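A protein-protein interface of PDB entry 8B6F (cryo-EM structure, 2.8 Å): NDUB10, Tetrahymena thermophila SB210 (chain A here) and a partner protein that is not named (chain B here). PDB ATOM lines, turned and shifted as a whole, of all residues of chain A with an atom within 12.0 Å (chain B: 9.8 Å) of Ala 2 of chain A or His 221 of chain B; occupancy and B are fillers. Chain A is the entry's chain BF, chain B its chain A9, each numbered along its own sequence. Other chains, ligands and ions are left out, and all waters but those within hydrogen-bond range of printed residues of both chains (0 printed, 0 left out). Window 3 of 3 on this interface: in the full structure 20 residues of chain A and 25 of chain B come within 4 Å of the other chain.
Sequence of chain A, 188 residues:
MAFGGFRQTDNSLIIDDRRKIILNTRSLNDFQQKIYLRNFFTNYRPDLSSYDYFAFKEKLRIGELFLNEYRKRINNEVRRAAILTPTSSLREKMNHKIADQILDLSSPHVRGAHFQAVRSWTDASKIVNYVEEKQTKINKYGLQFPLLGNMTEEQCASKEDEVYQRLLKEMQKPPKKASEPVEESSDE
The backbone NH of Ala 2 of chain A lies close to a ring nitrogen (NE2) of His 221 of chain B.
The guanidinium group of Arg 224 of chain B lies within hydrogen-bond range of the backbone carbonyl oxygen of Gly 218 of chain B (3.0 Å).
The backbone carbonyl oxygen (O) of Asn 219 of chain B sits at hydrogen-bond distance from the guanidinium group (NH2) of Arg 224 of chain B, at 2.4 Å.
The side-chain amide oxygen (OD1) of Asn 225 of chain B lies close to the backbone carbonyl oxygen (O) of His 221 of chain B.
The backbone NH of Phe 31 of chain A sits at hydrogen-bond distance from the side-chain amide oxygen of Asn 29 of chain A, at 3.2 Å.
Among the printed residues, pairs that only touch across the chains: Ala 2 of chain A with Asn 219 of chain B, Ala 2 of chain A with Tyr 220 of chain B, Phe 3 of chain A with Asn 219 of chain B, Phe 3 of chain A with His 221 of chain B, Phe 3 of chain A with Arg 224 of chain B and Phe 31 of chain A with Phe 216 of chain B.
Printed residues of chain B within 4 Å of Ala 2 of chain A: Asn 219, Tyr 220 and His 221.
His 221 of chain B touches just these residues of chain A: Ala 2 (3.3 Å) and Phe 3 (3.6 Å).
Phe 3 of chain A touches just these residues of chain B: Asn 219, His 221 and Arg 224.
No residue of chain A comes within 4 Å of Gly 218 of chain B.
Asn 219 of chain B touches two residues of chain A.
Lys 222 of chain B touches none of the printed residues of chain A.
Of the printed residues of chain B, Phe 31 of chain A touches Phe 216 (3.6 Å).
Of the printed residues of chain A, Phe 216 of chain B touches Phe 31 (3.6 Å).
Gly 5 of chain A touches none of the printed residues of chain B.
Leu 228 of chain B touches none of the printed residues of chain A.
The nearest printed residue of chain B that does not touch Phe 31 of chain A is Asn 219 of chain B (4.3 Å).
Hydrophobic or aromatic side chains of chain A that line the printed part of chain B: Ala 2, Phe 3 and Phe 31.
Hydrophobic or aromatic side chains of chain B within 4 Å of the printed part of chain A: Phe 216, Tyr 220 and His 221.
Along chain B the printed residues that touch a printed residue of chain A span positions 216 to 224.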
ATOM      1  N   ALA A   2     -14.106  29.997 -15.855  1.00  0.00           N
ATOM      2  CA  ALA A   2     -14.857  29.627 -14.624  1.00  0.00           C
ATOM      3  C   ALA A   2     -15.524  28.265 -14.772  1.00  0.00           C
ATOM      4  O   ALA A   2     -16.067  27.947 -15.828  1.00  0.00           O
ATOM      5  CB  ALA A   2     -15.892  30.681 -14.311  1.00  0.00           C
ATOM      6  N   PHE A   3     -15.481  27.463 -13.712  1.00  0.00           N
ATOM      7  CA  PHE A   3     -16.138  26.164 -13.734  1.00  0.00           C
ATOM      8  C   PHE A   3     -17.650  26.333 -13.810  1.00  0.00           C
ATOM      9  O   PHE A   3     -18.216  27.315 -13.325  1.00  0.00           O
ATOM     10  CB  PHE A   3     -15.781  25.350 -12.487  1.00  0.00           C
ATOM     11  CG  PHE A   3     -14.399  24.754 -12.510  1.00  0.00           C
ATOM     12  CD1 PHE A   3     -13.853  24.255 -13.682  1.00  0.00           C
ATOM     13  CD2 PHE A   3     -13.649  24.685 -11.349  1.00  0.00           C
ATOM     14  CE1 PHE A   3     -12.590  23.702 -13.696  1.00  0.00           C
ATOM     15  CE2 PHE A   3     -12.386  24.133 -11.356  1.00  0.00           C
ATOM     16  CZ  PHE A   3     -11.855  23.642 -12.532  1.00  0.00           C
ATOM     17  N   GLY A   4     -18.302  25.354 -14.430  1.00  0.00           N
ATOM     18  CA  GLY A   4     -19.745  25.357 -14.556  1.00  0.00           C
ATOM     19  C   GLY A   4     -20.365  24.073 -14.052  1.00  0.00           C
ATOM     20  O   GLY A   4     -19.759  23.358 -13.251  1.00  0.00           O
ATOM     21  N   GLY A   5     -21.579  23.770 -14.509  1.00  0.00           N
ATOM     22  CA  GLY A   5     -22.256  22.559 -14.093  1.00  0.00           C
ATOM     23  C   GLY A   5     -23.172  22.046 -15.181  1.00  0.00           C
ATOM     24  O   GLY A   5     -23.375  22.690 -16.212  1.00  0.00           O
ATOM     25  N   PHE A   6     -23.723  20.862 -14.935  1.00  0.00           N
ATOM     26  CA  PHE A   6     -24.648  20.209 -15.848  1.00  0.00           C
ATOM     27  C   PHE A   6     -25.989  20.063 -15.146  1.00  0.00           C
ATOM     28  O   PHE A   6     -26.044  19.642 -13.987  1.00  0.00           O
ATOM     29  CB  PHE A   6     -24.114  18.842 -16.285  1.00  0.00           C
ATOM     30  CG  PHE A   6     -24.814  18.268 -17.481  1.00  0.00           C
ATOM     31  CD1 PHE A   6     -26.015  17.593 -17.345  1.00  0.00           C
ATOM     32  CD2 PHE A   6     -24.256  18.386 -18.743  1.00  0.00           C
ATOM     33  CE1 PHE A   6     -26.655  17.058 -18.447  1.00  0.00           C
ATOM     34  CE2 PHE A   6     -24.889  17.854 -19.849  1.00  0.00           C
ATOM     35  CZ  PHE A   6     -26.090  17.187 -19.701  1.00  0.00           C
ATOM     36  N   ASN A  29     -27.789  25.170  -9.008  1.00  0.00           N
ATOM     37  CA  ASN A  29     -27.030  25.887 -10.021  1.00  0.00           C
ATOM     38  C   ASN A  29     -25.595  25.359 -10.027  1.00  0.00           C
ATOM     39  O   ASN A  29     -25.278  24.357  -9.381  1.00  0.00           O
ATOM     40  CB  ASN A  29     -27.102  27.396  -9.780  1.00  0.00           C
ATOM     41  CG  ASN A  29     -26.501  27.813  -8.454  1.00  0.00           C
ATOM     42  OD1 ASN A  29     -25.654  27.123  -7.895  1.00  0.00           O
ATOM     43  ND2 ASN A  29     -26.937  28.959  -7.946  1.00  0.00           N
ATOM     44  N   ASP A  30     -24.705  26.029 -10.758  1.00  0.00           N
ATOM     45  CA  ASP A  30     -23.343  25.525 -10.908  1.00  0.00           C
ATOM     46  C   ASP A  30     -22.602  25.522  -9.576  1.00  0.00           C
ATOM     47  O   ASP A  30     -21.975  24.524  -9.204  1.00  0.00           O
ATOM     48  CB  ASP A  30     -22.590  26.359 -11.942  1.00  0.00           C
ATOM     49  CG  ASP A  30     -23.289  26.386 -13.286  1.00  0.00           C
ATOM     50  OD1 ASP A  30     -24.346  27.042 -13.394  1.00  0.00           O
ATOM     51  OD2 ASP A  30     -22.786  25.745 -14.231  1.00  0.00           O
ATOM     52  N   PHE A  31     -22.648  26.638  -8.846  1.00  0.00           N
ATOM     53  CA  PHE A  31     -21.921  26.710  -7.582  1.00  0.00           C
ATOM     54  C   PHE A  31     -22.508  25.759  -6.546  1.00  0.00           C
ATOM     55  O   PHE A  31     -21.766  25.094  -5.815  1.00  0.00           O
ATOM     56  CB  PHE A  31     -21.924  28.140  -7.051  1.00  0.00           C
ATOM     57  CG  PHE A  31     -21.356  28.264  -5.672  1.00  0.00           C
ATOM     58  CD1 PHE A  31     -20.022  27.985  -5.431  1.00  0.00           C
ATOM     59  CD2 PHE A  31     -22.157  28.654  -4.613  1.00  0.00           C
ATOM     60  CE1 PHE A  31     -19.498  28.094  -4.162  1.00  0.00           C
ATOM     61  CE2 PHE A  31     -21.638  28.765  -3.341  1.00  0.00           C
ATOM     62  CZ  PHE A  31     -20.305  28.484  -3.114  1.00  0.00           C
ATOM     63  N   GLN A  33     -24.080  22.971  -7.159  1.00  0.00           N
ATOM     64  CA  GLN A  33     -23.642  21.639  -7.557  1.00  0.00           C
ATOM     65  C   GLN A  33     -22.212  21.383  -7.103  1.00  0.00           C
ATOM     66  O   GLN A  33     -21.902  20.317  -6.562  1.00  0.00           O
ATOM     67  CB  GLN A  33     -23.759  21.479  -9.073  1.00  0.00           C
ATOM     68  CG  GLN A  33     -25.180  21.355  -9.578  1.00  0.00           C
ATOM     69  CD  GLN A  33     -25.259  21.425 -11.085  1.00  0.00           C
ATOM     70  OE1 GLN A  33     -24.289  21.138 -11.781  1.00  0.00           O
ATOM     71  NE2 GLN A  33     -26.419  21.810 -11.599  1.00  0.00           N
ATOM     72  N   LYS A  34     -21.327  22.359  -7.307  1.00  0.00           N
ATOM     73  CA  LYS A  34     -19.944  22.210  -6.863  1.00  0.00           C
ATOM     74  C   LYS A  34     -19.874  21.971  -5.360  1.00  0.00           C
ATOM     75  O   LYS A  34     -19.106  21.122  -4.896  1.00  0.00           O
ATOM     76  CB  LYS A  34     -19.147  23.458  -7.251  1.00  0.00           C
ATOM     77  CG  LYS A  34     -17.776  23.594  -6.592  1.00  0.00           C
ATOM     78  CD  LYS A  34     -16.822  22.485  -7.003  1.00  0.00           C
ATOM     79  CE  LYS A  34     -16.343  22.670  -8.433  1.00  0.00           C
ATOM     80  NZ  LYS A  34     -15.294  21.677  -8.793  1.00  0.00           N
ATOM     81  N   ARG A  38     -20.001  16.733  -6.380  1.00  0.00           N
ATOM     82  CA  ARG A  38     -18.635  16.918  -6.855  1.00  0.00           C
ATOM     83  C   ARG A  38     -17.640  17.185  -5.735  1.00  0.00           C
ATOM     84  O   ARG A  38     -16.454  17.380  -6.021  1.00  0.00           O
ATOM     85  CB  ARG A  38     -18.529  18.067  -7.867  1.00  0.00           C
ATOM     86  CG  ARG A  38     -19.481  17.955  -9.044  1.00  0.00           C
ATOM     87  CD  ARG A  38     -19.221  19.053 -10.061  1.00  0.00           C
ATOM     88  NE  ARG A  38     -19.715  18.695 -11.386  1.00  0.00           N
ATOM     89  CZ  ARG A  38     -20.919  18.991 -11.854  1.00  0.00           C
ATOM     90  NH1 ARG A  38     -21.799  19.661 -11.130  1.00  0.00           N
ATOM     91  NH2 ARG A  38     -21.249  18.602 -13.081  1.00  0.00           N
ATOM     92  N   PHE B 216     -16.491  30.458  -3.819  1.00  0.00           N
ATOM     93  CA  PHE B 216     -16.883  30.504  -5.223  1.00  0.00           C
ATOM     94  C   PHE B 216     -15.829  31.190  -6.078  1.00  0.00           C
ATOM     95  O   PHE B 216     -15.644  30.824  -7.243  1.00  0.00           O
ATOM     96  CB  PHE B 216     -18.229  31.219  -5.350  1.00  0.00           C
ATOM     97  CG  PHE B 216     -18.489  31.795  -6.709  1.00  0.00           C
ATOM     98  CD1 PHE B 216     -18.990  31.002  -7.727  1.00  0.00           C
ATOM     99  CD2 PHE B 216     -18.257  33.137  -6.962  1.00  0.00           C
ATOM    100  CE1 PHE B 216     -19.239  31.533  -8.977  1.00  0.00           C
ATOM    101  CE2 PHE B 216     -18.505  33.673  -8.208  1.00  0.00           C
ATOM    102  CZ  PHE B 216     -18.996  32.870  -9.217  1.00  0.00           C
ATOM    103  N   LEU B 217     -15.131  32.184  -5.524  1.00  0.00           N
ATOM    104  CA  LEU B 217     -14.079  32.856  -6.279  1.00  0.00           C
ATOM    105  C   LEU B 217     -13.075  31.857  -6.835  1.00  0.00           C
ATOM    106  O   LEU B 217     -12.592  32.014  -7.961  1.00  0.00           O
ATOM    107  CB  LEU B 217     -13.373  33.885  -5.394  1.00  0.00           C
ATOM    108  CG  LEU B 217     -14.127  35.193  -5.140  1.00  0.00           C
ATOM    109  CD1 LEU B 217     -13.387  36.042  -4.128  1.00  0.00           C
ATOM    110  CD2 LEU B 217     -14.325  35.971  -6.429  1.00  0.00           C
ATOM    111  N   GLY B 218     -12.776  30.804  -6.077  1.00  0.00           N
ATOM    112  CA  GLY B 218     -11.818  29.811  -6.531  1.00  0.00           C
ATOM    113  C   GLY B 218     -12.227  29.105  -7.805  1.00  0.00           C
ATOM    114  O   GLY B 218     -11.382  28.483  -8.456  1.00  0.00           O
ATOM    115  N   ASN B 219     -13.507  29.178  -8.178  1.00  0.00           N
ATOM    116  CA  ASN B 219     -13.946  28.553  -9.420  1.00  0.00           C
ATOM    117  C   ASN B 219     -13.264  29.186 -10.626  1.00  0.00           C
ATOM    118  O   ASN B 219     -12.880  28.484 -11.569  1.00  0.00           O
ATOM    119  CB  ASN B 219     -15.463  28.654  -9.553  1.00  0.00           C
ATOM    120  CG  ASN B 219     -16.193  27.736  -8.596  1.00  0.00           C
ATOM    121  OD1 ASN B 219     -15.600  27.190  -7.667  1.00  0.00           O
ATOM    122  ND2 ASN B 219     -17.489  27.559  -8.819  1.00  0.00           N
ATOM    123  N   TYR B 220     -13.112  30.508 -10.620  1.00  0.00           N
ATOM    124  CA  TYR B 220     -12.451  31.187 -11.727  1.00  0.00           C
ATOM    125  C   TYR B 220     -11.033  30.659 -11.903  1.00  0.00           C
ATOM    126  O   TYR B 220     -10.286  30.512 -10.933  1.00  0.00           O
ATOM    127  CB  TYR B 220     -12.432  32.695 -11.478  1.00  0.00           C
ATOM    128  CG  TYR B 220     -13.799  33.321 -11.532  1.00  0.00           C
ATOM    129  CD1 TYR B 220     -14.439  33.527 -12.743  1.00  0.00           C
ATOM    130  CD2 TYR B 220     -14.452  33.705 -10.371  1.00  0.00           C
ATOM    131  CE1 TYR B 220     -15.691  34.095 -12.797  1.00  0.00           C
ATOM    132  CE2 TYR B 220     -15.703  34.274 -10.414  1.00  0.00           C
ATOM    133  CZ  TYR B 220     -16.320  34.461 -11.630  1.00  0.00           C
ATOM    134  OH  TYR B 220     -17.567  35.030 -11.679  1.00  0.00           O
ATOM    135  N   HIS B 221     -10.660  30.387 -13.152  1.00  0.00           N
ATOM    136  CA  HIS B 221      -9.346  29.810 -13.419  1.00  0.00           C
ATOM    137  C   HIS B 221      -8.239  30.825 -13.176  1.00  0.00           C
ATOM    138  O   HIS B 221      -7.175  30.478 -12.654  1.00  0.00           O
ATOM    139  CB  HIS B 221      -9.279  29.280 -14.851  1.00  0.00           C
ATOM    140  CG  HIS B 221     -10.478  28.483 -15.258  1.00  0.00           C
ATOM    141  ND1 HIS B 221     -10.906  28.402 -16.565  1.00  0.00           N
ATOM    142  CD2 HIS B 221     -11.341  27.733 -14.534  1.00  0.00           C
ATOM    143  CE1 HIS B 221     -11.979  27.636 -16.628  1.00  0.00           C
ATOM    144  NE2 HIS B 221     -12.265  27.218 -15.410  1.00  0.00           N
ATOM    145  N   LYS B 222      -8.467  32.083 -13.556  1.00  0.00           N
ATOM    146  CA  LYS B 222      -7.423  33.093 -13.437  1.00  0.00           C
ATOM    147  C   LYS B 222      -7.032  33.317 -11.980  1.00  0.00           C
ATOM    148  O   LYS B 222      -5.843  33.394 -11.651  1.00  0.00           O
ATOM    149  CB  LYS B 222      -7.889  34.401 -14.078  1.00  0.00           C
ATOM    150  CG  LYS B 222      -8.027  34.337 -15.591  1.00  0.00           C
ATOM    151  CD  LYS B 222      -6.672  34.180 -16.266  1.00  0.00           C
ATOM    152  CE  LYS B 222      -6.795  34.286 -17.777  1.00  0.00           C
ATOM    153  NZ  LYS B 222      -5.473  34.166 -18.451  1.00  0.00           N
ATOM    154  N   VAL B 223      -8.018  33.430 -11.089  1.00  0.00           N
ATOM    155  CA  VAL B 223      -7.703  33.659  -9.683  1.00  0.00           C
ATOM    156  C   VAL B 223      -7.053  32.423  -9.073  1.00  0.00           C
ATOM    157  O   VAL B 223      -6.100  32.530  -8.292  1.00  0.00           O
ATOM    158  CB  VAL B 223      -8.965  34.077  -8.902  1.00  0.00           C
ATOM    159  CG1 VAL B 223      -9.618  35.288  -9.536  1.00  0.00           C
ATOM    160  CG2 VAL B 223      -9.946  32.936  -8.800  1.00  0.00           C
ATOM    161  N   ARG B 224      -7.550  31.233  -9.416  1.00  0.00           N
ATOM    162  CA  ARG B 224      -6.969  30.011  -8.870  1.00  0.00           C
ATOM    163  C   ARG B 224      -5.512  29.867  -9.281  1.00  0.00           C
ATOM    164  O   ARG B 224      -4.662  29.497  -8.463  1.00  0.00           O
ATOM    165  CB  ARG B 224      -7.770  28.794  -9.331  1.00  0.00           C
ATOM    166  CG  ARG B 224      -7.386  27.510  -8.613  1.00  0.00           C
ATOM    167  CD  ARG B 224      -7.993  26.282  -9.267  1.00  0.00           C
ATOM    168  NE  ARG B 224      -9.392  26.495  -9.618  1.00  0.00           N
ATOM    169  CZ  ARG B 224      -9.853  26.665 -10.851  1.00  0.00           C
ATOM    170  NH1 ARG B 224      -9.057  26.609 -11.907  1.00  0.00           N
ATOM    171  NH2 ARG B 224     -11.150  26.898 -11.029  1.00  0.00           N
ATOM    172  N   ASN B 225      -5.202  30.152 -10.542  1.00  0.00           N
ATOM    173  CA  ASN B 225      -3.841  30.028 -11.043  1.00  0.00           C
ATOM    174  C   ASN B 225      -2.995  31.264 -10.774  1.00  0.00           C
ATOM    175  O   ASN B 225      -1.797  31.246 -11.071  1.00  0.00           O
ATOM    176  CB  ASN B 225      -3.861  29.739 -12.545  1.00  0.00           C
ATOM    177  CG  ASN B 225      -4.690  28.520 -12.893  1.00  0.00           C
ATOM    178  OD1 ASN B 225      -5.602  28.590 -13.714  1.00  0.00           O
ATOM    179  ND2 ASN B 225      -4.378  27.394 -12.264  1.00  0.00           N
ATOM    180  N   GLY B 226      -3.573  32.326 -10.225  1.00  0.00           N
ATOM    181  CA  GLY B 226      -2.797  33.532  -9.992  1.00  0.00           C
ATOM    182  C   GLY B 226      -2.253  34.136 -11.268  1.00  0.00           C
ATOM    183  O   GLY B 226      -1.081  34.529 -11.317  1.00  0.00           O
ATOM    184  N   GLN B 227      -3.079  34.214 -12.307  1.00  0.00           N
ATOM    185  CA  GLN B 227      -2.679  34.714 -13.616  1.00  0.00           C
ATOM    186  C   GLN B 227      -3.440  35.986 -13.967  1.00  0.00           C
ATOM    187  O   GLN B 227      -3.891  36.171 -15.099  1.00  0.00           O
ATOM    188  CB  GLN B 227      -2.894  33.646 -14.685  1.00  0.00           C
ATOM    189  CG  GLN B 227      -2.074  32.386 -14.458  1.00  0.00           C
ATOM    190  CD  GLN B 227      -2.288  31.340 -15.534  1.00  0.00           C
ATOM    191  OE1 GLN B 227      -1.337  30.718 -16.004  1.00  0.00           O
ATOM    192  NE2 GLN B 227      -3.541  31.130 -15.920  1.00  0.00           N
ATOM    193  N   LEU B 228      -3.595  36.876 -12.992  1.00  0.00           N
ATOM    194  CA  LEU B 228      -4.279  38.145 -13.177  1.00  0.00           C
ATOM    195  C   LEU B 228      -3.278  39.290 -13.141  1.00  0.00           C
ATOM    196  O   LEU B 228      -2.360  39.299 -12.315  1.00  0.00           O
ATOM    197  CB  LEU B 228      -5.341  38.368 -12.096  1.00  0.00           C
ATOM    198  CG  LEU B 228      -6.611  37.521 -12.155  1.00  0.00           C
ATOM    199  CD1 LEU B 228      -7.489  37.845 -10.968  1.00  0.00           C
ATOM    200  CD2 LEU B 228      -7.372  37.741 -13.448  1.00  0.00           C
